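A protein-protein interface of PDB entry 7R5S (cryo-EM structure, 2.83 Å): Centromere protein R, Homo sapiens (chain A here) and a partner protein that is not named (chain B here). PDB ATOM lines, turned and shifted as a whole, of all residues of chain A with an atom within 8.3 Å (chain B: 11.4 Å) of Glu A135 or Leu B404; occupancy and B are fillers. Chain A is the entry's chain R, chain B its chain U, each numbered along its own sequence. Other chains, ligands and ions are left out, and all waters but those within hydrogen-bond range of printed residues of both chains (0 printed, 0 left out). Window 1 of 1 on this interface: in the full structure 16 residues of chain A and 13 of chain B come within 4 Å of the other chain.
Printed residues of chain A that touch a printed residue of chain B: Phe A131, Arg A134, Glu A135, Met A136, Lys A138, Thr A139 and Leu A142. Of the 19 printed residues of chain B, 5 touch a printed residue of chain A. Among the printed residues, no Asp or Glu carboxylate lies within 4 Å of a Lys or Arg side-chain nitrogen of the other chain.
Phe A131 touches Glu B401 (CE1 to CB, 3.99 Å). Arg B405 touches Phe A131 (CZ to CZ, 3.6 Å). NH2 of Arg A134 touches CD of Arg B405 (3.6 Å). CG of Glu A135 touches CB of Leu B404, at 3.5 Å. OE2 of Glu A135 touches CA of Arg B405 (3.2 Å). Leu B404 touches Met A136 (CD1 to CG, 3.7 Å). Asn B408 touches Lys A138 (OD1 to CE, 3.6 Å). Thr A139 touches Asn B408. CD1 of Leu A142 touches OE2 of Glu B412 (3.2 Å).
No residue of chain B comes within 4 Å of Leu A132. Arg A134 touches just one residue of chain B: Arg B405 (3.6 Å). Of chain B, only Leu B404, Arg B405 and Asn B408 come within 4 Å of Glu A135. Gln A137 touches none of the printed residues of chain B. Lys A138 touches one residue of chain B. Thr A139 touches just one residue of chain B: Asn B408. Of the printed residues of chain A, Leu B404 touches Glu A135 and Met A136. Asn B406 touches none of the printed residues of chain A. Of the printed residues of chain A, Asn B408 touches Glu A135, Lys A138 and Thr A139. Gln B410 touches none of the printed residues of chain A. Of the printed residues of chain A, Glu B412 touches Leu A142. The nearest residue of chain A that does not touch Leu B404 is Thr A139 (4.3 Å). The nearest printed residue of chain A that does not touch Arg B405 is Lys A138 (5.2 Å).
The side-chain amide oxygen (OD1) of Asn B408 sits close to the side-chain carboxylate (OE2) of Glu A135 (2.8 Å).
O of Glu B401 sits at hydrogen-bond distance from NE of Arg B405. The guanidinium group of Arg B405 is in hydrogen-bond range of the side-chain hydroxyl of Ser B402 (3.1 Å). The backbone carbonyl oxygen (O) of Leu B404 sits close to the side-chain amide oxygen (OD1) of Asn B408 (2.8 Å). O of Asn B408 lies close to OE2 of Glu B412 (2.7 Å). OE1 of Glu A135 is in salt-bridge range of NZ of Lys A138, at 3.0 Å. O of Met A136 is in hydrogen-bond range of OG1 of Thr A139 (3.4 Å).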
ATOM      1  N   LEU A  90      -4.727  11.210 -15.681  1.00  0.00           N
ATOM      2  CA  LEU A  90      -5.466  12.466 -15.633  1.00  0.00           C
ATOM      3  C   LEU A  90      -5.987  12.862 -17.006  1.00  0.00           C
ATOM      4  O   LEU A  90      -7.130  13.318 -17.127  1.00  0.00           O
ATOM      5  CB  LEU A  90      -4.579  13.582 -15.087  1.00  0.00           C
ATOM      6  CG  LEU A  90      -5.319  14.827 -14.607  1.00  0.00           C
ATOM      7  CD1 LEU A  90      -5.903  14.633 -13.209  1.00  0.00           C
ATOM      8  CD2 LEU A  90      -4.400  16.031 -14.685  1.00  0.00           C
ATOM      9  N   VAL A  93      -8.992  10.606 -17.855  1.00  0.00           N
ATOM     10  CA  VAL A  93     -10.210  10.898 -17.100  1.00  0.00           C
ATOM     11  C   VAL A  93     -10.785  12.248 -17.520  1.00  0.00           C
ATOM     12  O   VAL A  93     -12.009  12.438 -17.512  1.00  0.00           O
ATOM     13  CB  VAL A  93      -9.971  10.839 -15.577  1.00  0.00           C
ATOM     14  CG1 VAL A  93      -9.616   9.423 -15.137  1.00  0.00           C
ATOM     15  CG2 VAL A  93      -8.932  11.842 -15.131  1.00  0.00           C
ATOM     16  N   GLU A  94      -9.935  13.192 -17.936  1.00  0.00           N
ATOM     17  CA  GLU A  94     -10.454  14.453 -18.455  1.00  0.00           C
ATOM     18  C   GLU A  94     -11.199  14.255 -19.769  1.00  0.00           C
ATOM     19  O   GLU A  94     -12.267  14.846 -19.967  1.00  0.00           O
ATOM     20  CB  GLU A  94      -9.318  15.458 -18.637  1.00  0.00           C
ATOM     21  CG  GLU A  94      -9.766  16.880 -18.969  1.00  0.00           C
ATOM     22  CD  GLU A  94     -10.897  17.384 -18.085  1.00  0.00           C
ATOM     23  OE1 GLU A  94     -12.075  17.112 -18.399  1.00  0.00           O
ATOM     24  OE2 GLU A  94     -10.608  18.067 -17.082  1.00  0.00           O
ATOM     25  N   ILE A 100     -18.965  10.920 -19.353  1.00  0.00           N
ATOM     26  CA  ILE A 100     -19.648  10.585 -18.104  1.00  0.00           C
ATOM     27  C   ILE A 100     -20.743  11.604 -17.818  1.00  0.00           C
ATOM     28  O   ILE A 100     -21.816  11.246 -17.311  1.00  0.00           O
ATOM     29  CB  ILE A 100     -18.686  10.456 -16.906  1.00  0.00           C
ATOM     30  CG1 ILE A 100     -17.875  11.728 -16.690  1.00  0.00           C
ATOM     31  CG2 ILE A 100     -17.759   9.270 -17.092  1.00  0.00           C
ATOM     32  CD1 ILE A 100     -16.882  11.635 -15.559  1.00  0.00           C
ATOM     33  N   HIS A 130     -23.377  19.062 -11.295  1.00  0.00           N
ATOM     34  CA  HIS A 130     -23.579  19.928 -12.447  1.00  0.00           C
ATOM     35  C   HIS A 130     -22.419  20.877 -12.707  1.00  0.00           C
ATOM     36  O   HIS A 130     -22.202  21.257 -13.862  1.00  0.00           O
ATOM     37  CB  HIS A 130     -24.864  20.752 -12.280  1.00  0.00           C
ATOM     38  CG  HIS A 130     -26.117  19.936 -12.350  1.00  0.00           C
ATOM     39  ND1 HIS A 130     -26.507  19.084 -11.339  1.00  0.00           N
ATOM     40  CD2 HIS A 130     -27.062  19.836 -13.313  1.00  0.00           C
ATOM     41  CE1 HIS A 130     -27.642  18.498 -11.675  1.00  0.00           C
ATOM     42  NE2 HIS A 130     -28.001  18.937 -12.869  1.00  0.00           N
ATOM     43  N   PHE A 131     -21.674  21.264 -11.671  1.00  0.00           N
ATOM     44  CA  PHE A 131     -20.467  22.068 -11.815  1.00  0.00           C
ATOM     45  C   PHE A 131     -19.220  21.208 -11.973  1.00  0.00           C
ATOM     46  O   PHE A 131     -18.113  21.655 -11.642  1.00  0.00           O
ATOM     47  CB  PHE A 131     -20.321  23.005 -10.616  1.00  0.00           C
ATOM     48  CG  PHE A 131     -20.456  22.313  -9.290  1.00  0.00           C
ATOM     49  CD1 PHE A 131     -19.357  21.727  -8.685  1.00  0.00           C
ATOM     50  CD2 PHE A 131     -21.682  22.245  -8.650  1.00  0.00           C
ATOM     51  CE1 PHE A 131     -19.478  21.087  -7.467  1.00  0.00           C
ATOM     52  CE2 PHE A 131     -21.809  21.606  -7.431  1.00  0.00           C
ATOM     53  CZ  PHE A 131     -20.705  21.027  -6.839  1.00  0.00           C
ATOM     54  N   LEU A 132     -19.382  19.977 -12.466  1.00  0.00           N
ATOM     55  CA  LEU A 132     -18.261  19.051 -12.583  1.00  0.00           C
ATOM     56  C   LEU A 132     -17.170  19.603 -13.494  1.00  0.00           C
ATOM     57  O   LEU A 132     -15.987  19.290 -13.304  1.00  0.00           O
ATOM     58  CB  LEU A 132     -18.775  17.698 -13.079  1.00  0.00           C
ATOM     59  CG  LEU A 132     -18.003  16.422 -12.739  1.00  0.00           C
ATOM     60  CD1 LEU A 132     -18.938  15.226 -12.779  1.00  0.00           C
ATOM     61  CD2 LEU A 132     -16.857  16.208 -13.705  1.00  0.00           C
ATOM     62  N   LYS A 133     -17.545  20.430 -14.478  1.00  0.00           N
ATOM     63  CA  LYS A 133     -16.552  21.104 -15.309  1.00  0.00           C
ATOM     64  C   LYS A 133     -15.561  21.876 -14.449  1.00  0.00           C
ATOM     65  O   LYS A 133     -14.341  21.707 -14.575  1.00  0.00           O
ATOM     66  CB  LYS A 133     -17.235  22.065 -16.289  1.00  0.00           C
ATOM     67  CG  LYS A 133     -18.547  21.611 -16.922  1.00  0.00           C
ATOM     68  CD  LYS A 133     -18.472  20.224 -17.527  1.00  0.00           C
ATOM     69  CE  LYS A 133     -19.865  19.683 -17.812  1.00  0.00           C
ATOM     70  NZ  LYS A 133     -20.724  19.662 -16.597  1.00  0.00           N
ATOM     71  N   ARG A 134     -16.079  22.729 -13.561  1.00  0.00           N
ATOM     72  CA  ARG A 134     -15.236  23.592 -12.739  1.00  0.00           C
ATOM     73  C   ARG A 134     -14.262  22.777 -11.898  1.00  0.00           C
ATOM     74  O   ARG A 134     -13.058  23.048 -11.879  1.00  0.00           O
ATOM     75  CB  ARG A 134     -16.114  24.480 -11.851  1.00  0.00           C
ATOM     76  CG  ARG A 134     -15.343  25.318 -10.839  1.00  0.00           C
ATOM     77  CD  ARG A 134     -16.249  25.820  -9.722  1.00  0.00           C
ATOM     78  NE  ARG A 134     -16.861  24.728  -8.968  1.00  0.00           N
ATOM     79  CZ  ARG A 134     -16.724  24.555  -7.656  1.00  0.00           C
ATOM     80  NH1 ARG A 134     -15.997  25.404  -6.943  1.00  0.00           N
ATOM     81  NH2 ARG A 134     -17.315  23.531  -7.056  1.00  0.00           N
ATOM     82  N   GLU A 135     -14.764  21.760 -11.199  1.00  0.00           N
ATOM     83  CA  GLU A 135     -13.908  21.005 -10.289  1.00  0.00           C
ATOM     84  C   GLU A 135     -12.884  20.167 -11.047  1.00  0.00           C
ATOM     85  O   GLU A 135     -11.702  20.140 -10.676  1.00  0.00           O
ATOM     86  CB  GLU A 135     -14.762  20.124  -9.377  1.00  0.00           C
ATOM     87  CG  GLU A 135     -14.160  19.904  -8.000  1.00  0.00           C
ATOM     88  CD  GLU A 135     -14.155  21.162  -7.154  1.00  0.00           C
ATOM     89  OE1 GLU A 135     -14.998  22.051  -7.393  1.00  0.00           O
ATOM     90  OE2 GLU A 135     -13.304  21.263  -6.247  1.00  0.00           O
ATOM     91  N   MET A 136     -13.308  19.482 -12.112  1.00  0.00           N
ATOM     92  CA  MET A 136     -12.373  18.639 -12.847  1.00  0.00           C
ATOM     93  C   MET A 136     -11.359  19.443 -13.645  1.00  0.00           C
ATOM     94  O   MET A 136     -10.290  18.912 -13.969  1.00  0.00           O
ATOM     95  CB  MET A 136     -13.122  17.685 -13.776  1.00  0.00           C
ATOM     96  CG  MET A 136     -13.400  16.333 -13.148  1.00  0.00           C
ATOM     97  SD  MET A 136     -11.888  15.416 -12.796  1.00  0.00           S
ATOM     98  CE  MET A 136     -11.879  14.251 -14.156  1.00  0.00           C
ATOM     99  N   GLN A 137     -11.654  20.702 -13.967  1.00  0.00           N
ATOM    100  CA  GLN A 137     -10.643  21.567 -14.554  1.00  0.00           C
ATOM    101  C   GLN A 137      -9.801  22.286 -13.509  1.00  0.00           C
ATOM    102  O   GLN A 137      -8.695  22.736 -13.828  1.00  0.00           O
ATOM    103  CB  GLN A 137     -11.297  22.597 -15.484  1.00  0.00           C
ATOM    104  CG  GLN A 137     -11.544  22.113 -16.917  1.00  0.00           C
ATOM    105  CD  GLN A 137     -12.674  21.104 -17.047  1.00  0.00           C
ATOM    106  OE1 GLN A 137     -12.765  20.141 -16.285  1.00  0.00           O
ATOM    107  NE2 GLN A 137     -13.546  21.324 -18.025  1.00  0.00           N
ATOM    108  N   LYS A 138     -10.295  22.403 -12.273  1.00  0.00           N
ATOM    109  CA  LYS A 138      -9.512  23.037 -11.221  1.00  0.00           C
ATOM    110  C   LYS A 138      -8.485  22.085 -10.626  1.00  0.00           C
ATOM    111  O   LYS A 138      -7.399  22.523 -10.231  1.00  0.00           O
ATOM    112  CB  LYS A 138     -10.435  23.572 -10.126  1.00  0.00           C
ATOM    113  CG  LYS A 138      -9.713  24.343  -9.032  1.00  0.00           C
ATOM    114  CD  LYS A 138     -10.670  24.801  -7.947  1.00  0.00           C
ATOM    115  CE  LYS A 138     -11.524  23.653  -7.440  1.00  0.00           C
ATOM    116  NZ  LYS A 138     -12.884  24.114  -7.048  1.00  0.00           N
ATOM    117  N   THR A 139      -8.803  20.789 -10.547  1.00  0.00           N
ATOM    118  CA  THR A 139      -7.825  19.838 -10.017  1.00  0.00           C
ATOM    119  C   THR A 139      -6.553  19.790 -10.857  1.00  0.00           C
ATOM    120  O   THR A 139      -5.511  19.335 -10.369  1.00  0.00           O
ATOM    121  CB  THR A 139      -8.419  18.429  -9.910  1.00  0.00           C
ATOM    122  OG1 THR A 139      -8.592  17.867 -11.220  1.00  0.00           O
ATOM    123  CG2 THR A 139      -9.734  18.435  -9.151  1.00  0.00           C
ATOM    124  N   LYS A 140      -6.611  20.258 -12.108  1.00  0.00           N
ATOM    125  CA  LYS A 140      -5.476  20.105 -13.014  1.00  0.00           C
ATOM    126  C   LYS A 140      -4.270  20.931 -12.579  1.00  0.00           C
ATOM    127  O   LYS A 140      -3.156  20.395 -12.493  1.00  0.00           O
ATOM    128  CB  LYS A 140      -5.884  20.491 -14.437  1.00  0.00           C
ATOM    129  CG  LYS A 140      -7.088  19.743 -14.995  1.00  0.00           C
ATOM    130  CD  LYS A 140      -7.053  18.279 -14.611  1.00  0.00           C
ATOM    131  CE  LYS A 140      -7.939  17.447 -15.510  1.00  0.00           C
ATOM    132  NZ  LYS A 140      -7.154  16.880 -16.636  1.00  0.00           N
ATOM    133  N   GLU A 141      -4.462  22.224 -12.301  1.00  0.00           N
ATOM    134  CA  GLU A 141      -3.331  23.053 -11.895  1.00  0.00           C
ATOM    135  C   GLU A 141      -2.765  22.593 -10.556  1.00  0.00           C
ATOM    136  O   GLU A 141      -1.544  22.609 -10.353  1.00  0.00           O
ATOM    137  CB  GLU A 141      -3.733  24.529 -11.837  1.00  0.00           C
ATOM    138  CG  GLU A 141      -5.022  24.822 -11.089  1.00  0.00           C
ATOM    139  CD  GLU A 141      -6.242  24.771 -11.989  1.00  0.00           C
ATOM    140  OE1 GLU A 141      -6.157  24.172 -13.081  1.00  0.00           O
ATOM    141  OE2 GLU A 141      -7.287  25.335 -11.603  1.00  0.00           O
ATOM    142  N   LEU A 142      -3.632  22.155  -9.640  1.00  0.00           N
ATOM    143  CA  LEU A 142      -3.148  21.661  -8.356  1.00  0.00           C
ATOM    144  C   LEU A 142      -2.335  20.379  -8.512  1.00  0.00           C
ATOM    145  O   LEU A 142      -1.275  20.245  -7.889  1.00  0.00           O
ATOM    146  CB  LEU A 142      -4.319  21.445  -7.394  1.00  0.00           C
ATOM    147  CG  LEU A 142      -4.939  22.695  -6.751  1.00  0.00           C
ATOM    148  CD1 LEU A 142      -3.849  23.588  -6.172  1.00  0.00           C
ATOM    149  CD2 LEU A 142      -5.825  23.480  -7.704  1.00  0.00           C
ATOM    150  N   ARG B 395     -23.760   6.339  -4.422  1.00  0.00           N
ATOM    151  CA  ARG B 395     -23.499   7.485  -3.559  1.00  0.00           C
ATOM    152  C   ARG B 395     -22.215   8.198  -3.965  1.00  0.00           C
ATOM    153  O   ARG B 395     -22.222   9.397  -4.267  1.00  0.00           O
ATOM    154  CB  ARG B 395     -23.425   7.031  -2.100  1.00  0.00           C
ATOM    155  CG  ARG B 395     -22.817   8.058  -1.165  1.00  0.00           C
ATOM    156  CD  ARG B 395     -22.444   7.432   0.165  1.00  0.00           C
ATOM    157  NE  ARG B 395     -21.745   8.375   1.031  1.00  0.00           N
ATOM    158  CZ  ARG B 395     -21.272   8.075   2.235  1.00  0.00           C
ATOM    159  NH1 ARG B 395     -21.421   6.851   2.722  1.00  0.00           N
ATOM    160  NH2 ARG B 395     -20.649   8.999   2.954  1.00  0.00           N
ATOM    161  N   THR B 396     -21.097   7.468  -3.977  1.00  0.00           N
ATOM    162  CA  THR B 396     -19.834   8.061  -4.405  1.00  0.00           C
ATOM    163  C   THR B 396     -19.871   8.455  -5.876  1.00  0.00           C
ATOM    164  O   THR B 396     -19.227   9.432  -6.271  1.00  0.00           O
ATOM    165  CB  THR B 396     -18.676   7.097  -4.141  1.00  0.00           C
ATOM    166  OG1 THR B 396     -17.484   7.597  -4.760  1.00  0.00           O
ATOM    167  CG2 THR B 396     -18.986   5.715  -4.694  1.00  0.00           C
ATOM    168  N   LEU B 397     -20.636   7.726  -6.692  1.00  0.00           N
ATOM    169  CA  LEU B 397     -20.763   8.072  -8.104  1.00  0.00           C
ATOM    170  C   LEU B 397     -21.290   9.493  -8.265  1.00  0.00           C
ATOM    171  O   LEU B 397     -20.729  10.297  -9.018  1.00  0.00           O
ATOM    172  CB  LEU B 397     -21.689   7.070  -8.795  1.00  0.00           C
ATOM    173  CG  LEU B 397     -21.858   7.017 -10.318  1.00  0.00           C
ATOM    174  CD1 LEU B 397     -22.543   5.705 -10.677  1.00  0.00           C
ATOM    175  CD2 LEU B 397     -22.606   8.205 -10.925  1.00  0.00           C
ATOM    176  N   LEU B 398     -22.373   9.815  -7.561  1.00  0.00           N
ATOM    177  CA  LEU B 398     -22.984  11.134  -7.667  1.00  0.00           C
ATOM    178  C   LEU B 398     -22.345  12.164  -6.741  1.00  0.00           C
ATOM    179  O   LEU B 398     -22.621  13.360  -6.891  1.00  0.00           O
ATOM    180  CB  LEU B 398     -24.491  11.049  -7.391  1.00  0.00           C
ATOM    181  CG  LEU B 398     -25.373  10.537  -8.540  1.00  0.00           C
ATOM    182  CD1 LEU B 398     -25.314   9.021  -8.676  1.00  0.00           C
ATOM    183  CD2 LEU B 398     -26.814  11.005  -8.401  1.00  0.00           C
ATOM    184  N   GLY B 399     -21.507  11.740  -5.799  1.00  0.00           N
ATOM    185  CA  GLY B 399     -20.764  12.649  -4.952  1.00  0.00           C
ATOM    186  C   GLY B 399     -19.308  12.821  -5.323  1.00  0.00           C
ATOM    187  O   GLY B 399     -18.544  13.384  -4.527  1.00  0.00           O
ATOM    188  N   ALA B 400     -18.886  12.307  -6.482  1.00  0.00           N
ATOM    189  CA  ALA B 400     -17.537  12.573  -6.970  1.00  0.00           C
ATOM    190  C   ALA B 400     -17.221  14.063  -7.013  1.00  0.00           C
ATOM    191  O   ALA B 400     -16.061  14.451  -6.858  1.00  0.00           O
ATOM    192  CB  ALA B 400     -17.352  11.954  -8.356  1.00  0.00           C
ATOM    193  N   GLU B 401     -18.230  14.914  -7.215  1.00  0.00           N
ATOM    194  CA  GLU B 401     -17.991  16.356  -7.192  1.00  0.00           C
ATOM    195  C   GLU B 401     -17.500  16.806  -5.821  1.00  0.00           C
ATOM    196  O   GLU B 401     -16.483  17.504  -5.709  1.00  0.00           O
ATOM    197  CB  GLU B 401     -19.265  17.105  -7.584  1.00  0.00           C
ATOM    198  N   SER B 402     -18.206  16.406  -4.762  1.00  0.00           N
ATOM    199  CA  SER B 402     -17.760  16.730  -3.412  1.00  0.00           C
ATOM    200  C   SER B 402     -16.442  16.045  -3.079  1.00  0.00           C
ATOM    201  O   SER B 402     -15.647  16.579  -2.300  1.00  0.00           O
ATOM    202  CB  SER B 402     -18.836  16.343  -2.398  1.00  0.00           C
ATOM    203  OG  SER B 402     -20.098  16.867  -2.774  1.00  0.00           O
ATOM    204  N   HIS B 403     -16.186  14.874  -3.665  1.00  0.00           N
ATOM    205  CA  HIS B 403     -14.919  14.190  -3.421  1.00  0.00           C
ATOM    206  C   HIS B 403     -13.746  14.963  -4.018  1.00  0.00           C
ATOM    207  O   HIS B 403     -12.692  15.098  -3.382  1.00  0.00           O
ATOM    208  CB  HIS B 403     -14.976  12.769  -3.979  1.00  0.00           C
ATOM    209  CG  HIS B 403     -15.992  11.899  -3.307  1.00  0.00           C
ATOM    210  ND1 HIS B 403     -16.382  10.679  -3.812  1.00  0.00           N
ATOM    211  CD2 HIS B 403     -16.699  12.076  -2.165  1.00  0.00           C
ATOM    212  CE1 HIS B 403     -17.286  10.141  -3.013  1.00  0.00           C
ATOM    213  NE2 HIS B 403     -17.495  10.968  -2.005  1.00  0.00           N
ATOM    214  N   LEU B 404     -13.909  15.482  -5.238  1.00  0.00           N
ATOM    215  CA  LEU B 404     -12.877  16.336  -5.816  1.00  0.00           C
ATOM    216  C   LEU B 404     -12.753  17.654  -5.062  1.00  0.00           C
ATOM    217  O   LEU B 404     -11.646  18.187  -4.931  1.00  0.00           O
ATOM    218  CB  LEU B 404     -13.144  16.591  -7.300  1.00  0.00           C
ATOM    219  CG  LEU B 404     -13.482  15.394  -8.185  1.00  0.00           C
ATOM    220  CD1 LEU B 404     -13.938  15.860  -9.551  1.00  0.00           C
ATOM    221  CD2 LEU B 404     -12.277  14.480  -8.315  1.00  0.00           C
ATOM    222  N   ARG B 405     -13.864  18.191  -4.555  1.00  0.00           N
ATOM    223  CA  ARG B 405     -13.778  19.361  -3.684  1.00  0.00           C
ATOM    224  C   ARG B 405     -12.915  19.063  -2.461  1.00  0.00           C
ATOM    225  O   ARG B 405     -12.052  19.864  -2.076  1.00  0.00           O
ATOM    226  CB  ARG B 405     -15.178  19.804  -3.261  1.00  0.00           C
ATOM    227  CG  ARG B 405     -15.691  21.035  -3.988  1.00  0.00           C
ATOM    228  CD  ARG B 405     -16.822  20.690  -4.947  1.00  0.00           C
ATOM    229  NE  ARG B 405     -17.921  19.999  -4.279  1.00  0.00           N
ATOM    230  CZ  ARG B 405     -18.952  20.613  -3.709  1.00  0.00           C
ATOM    231  NH1 ARG B 405     -19.026  21.937  -3.718  1.00  0.00           N
ATOM    232  NH2 ARG B 405     -19.911  19.905  -3.127  1.00  0.00           N
ATOM    233  N   ASN B 406     -13.132  17.896  -1.846  1.00  0.00           N
ATOM    234  CA  ASN B 406     -12.361  17.506  -0.671  1.00  0.00           C
ATOM    235  C   ASN B 406     -10.885  17.345  -1.002  1.00  0.00           C
ATOM    236  O   ASN B 406     -10.018  17.793  -0.241  1.00  0.00           O
ATOM    237  CB  ASN B 406     -12.913  16.207  -0.089  1.00  0.00           C
ATOM    238  CG  ASN B 406     -13.842  16.440   1.079  1.00  0.00           C
ATOM    239  OD1 ASN B 406     -13.502  17.146   2.027  1.00  0.00           O
ATOM    240  ND2 ASN B 406     -15.021  15.838   1.022  1.00  0.00           N
ATOM    241  N   ILE B 407     -10.575  16.690  -2.123  1.00  0.00           N
ATOM    242  CA  ILE B 407      -9.170  16.484  -2.457  1.00  0.00           C
ATOM    243  C   ILE B 407      -8.502  17.803  -2.821  1.00  0.00           C
ATOM    244  O   ILE B 407      -7.319  18.002  -2.540  1.00  0.00           O
ATOM    245  CB  ILE B 407      -8.992  15.433  -3.567  1.00  0.00           C
ATOM    246  CG1 ILE B 407      -7.504  15.139  -3.734  1.00  0.00           C
ATOM    247  CG2 ILE B 407      -9.532  15.924  -4.881  1.00  0.00           C
ATOM    248  CD1 ILE B 407      -7.208  13.806  -4.299  1.00  0.00           C
ATOM    249  N   ASN B 408      -9.241  18.738  -3.427  1.00  0.00           N
ATOM    250  CA  ASN B 408      -8.660  20.052  -3.691  1.00  0.00           C
ATOM    251  C   ASN B 408      -8.369  20.794  -2.392  1.00  0.00           C
ATOM    252  O   ASN B 408      -7.295  21.392  -2.236  1.00  0.00           O
ATOM    253  CB  ASN B 408      -9.591  20.875  -4.583  1.00  0.00           C
ATOM    254  CG  ASN B 408      -9.612  20.381  -6.018  1.00  0.00           C
ATOM    255  OD1 ASN B 408     -10.675  20.240  -6.623  1.00  0.00           O
ATOM    256  ND2 ASN B 408      -8.433  20.118  -6.569  1.00  0.00           N
ATOM    257  N   HIS B 409      -9.313  20.761  -1.450  1.00  0.00           N
ATOM    258  CA  HIS B 409      -9.095  21.406  -0.161  1.00  0.00           C
ATOM    259  C   HIS B 409      -7.872  20.819   0.534  1.00  0.00           C
ATOM    260  O   HIS B 409      -6.988  21.551   1.000  1.00  0.00           O
ATOM    261  CB  HIS B 409     -10.341  21.255   0.710  1.00  0.00           C
ATOM    262  CG  HIS B 409     -10.375  22.177   1.888  1.00  0.00           C
ATOM    263  ND1 HIS B 409      -9.627  21.958   3.025  1.00  0.00           N
ATOM    264  CD2 HIS B 409     -11.078  23.312   2.112  1.00  0.00           C
ATOM    265  CE1 HIS B 409      -9.864  22.922   3.897  1.00  0.00           C
ATOM    266  NE2 HIS B 409     -10.741  23.757   3.368  1.00  0.00           N
ATOM    267  N   GLN B 410      -7.790  19.491   0.585  1.00  0.00           N
ATOM    268  CA  GLN B 410      -6.660  18.836   1.226  1.00  0.00           C
ATOM    269  C   GLN B 410      -5.362  19.001   0.446  1.00  0.00           C
ATOM    270  O   GLN B 410      -4.291  18.985   1.056  1.00  0.00           O
ATOM    271  CB  GLN B 410      -6.961  17.347   1.432  1.00  0.00           C
ATOM    272  CG  GLN B 410      -6.169  16.691   2.567  1.00  0.00           C
ATOM    273  CD  GLN B 410      -6.528  17.219   3.952  1.00  0.00           C
ATOM    274  OE1 GLN B 410      -7.340  18.132   4.097  1.00  0.00           O
ATOM    275  NE2 GLN B 410      -5.911  16.643   4.977  1.00  0.00           N
ATOM    276  N   LEU B 411      -5.423  19.210  -0.870  1.00  0.00           N
ATOM    277  CA  LEU B 411      -4.202  19.428  -1.636  1.00  0.00           C
ATOM    278  C   LEU B 411      -3.643  20.817  -1.376  1.00  0.00           C
ATOM    279  O   LEU B 411      -2.425  20.985  -1.258  1.00  0.00           O
ATOM    280  CB  LEU B 411      -4.467  19.222  -3.127  1.00  0.00           C
ATOM    281  CG  LEU B 411      -4.266  17.796  -3.648  1.00  0.00           C
ATOM    282  CD1 LEU B 411      -4.481  17.726  -5.153  1.00  0.00           C
ATOM    283  CD2 LEU B 411      -2.884  17.279  -3.278  1.00  0.00           C
ATOM    284  N   GLU B 412      -4.515  21.824  -1.292  1.00  0.00           N
ATOM    285  CA  GLU B 412      -4.067  23.132  -0.822  1.00  0.00           C
ATOM    286  C   GLU B 412      -3.507  23.044   0.594  1.00  0.00           C
ATOM    287  O   GLU B 412      -2.450  23.619   0.890  1.00  0.00           O
ATOM    288  CB  GLU B 412      -5.214  24.143  -0.897  1.00  0.00           C
ATOM    289  CG  GLU B 412      -5.248  24.980  -2.180  1.00  0.00           C
ATOM    290  CD  GLU B 412      -5.826  24.250  -3.377  1.00  0.00           C
ATOM    291  OE1 GLU B 412      -6.514  24.904  -4.191  1.00  0.00           O
ATOM    292  OE2 GLU B 412      -5.576  23.036  -3.529  1.00  0.00           O
ATOM    293  N   LYS B 413      -4.196  22.313   1.476  1.00  0.00           N
ATOM    294  CA  LYS B 413      -3.696  22.116   2.834  1.00  0.00           C
ATOM    295  C   LYS B 413      -2.299  21.510   2.827  1.00  0.00           C
ATOM    296  O   LYS B 413      -1.444  21.886   3.636  1.00  0.00           O
ATOM    297  CB  LYS B 413      -4.657  21.223   3.620  1.00  0.00           C
ATOM    298  CG  LYS B 413      -4.576  21.398   5.128  1.00  0.00           C
ATOM    299  CD  LYS B 413      -4.775  22.846   5.532  1.00  0.00           C
ATOM    300  CE  LYS B 413      -6.222  23.270   5.344  1.00  0.00           C
ATOM    301  NZ  LYS B 413      -6.539  24.512   6.101  1.00  0.00           N
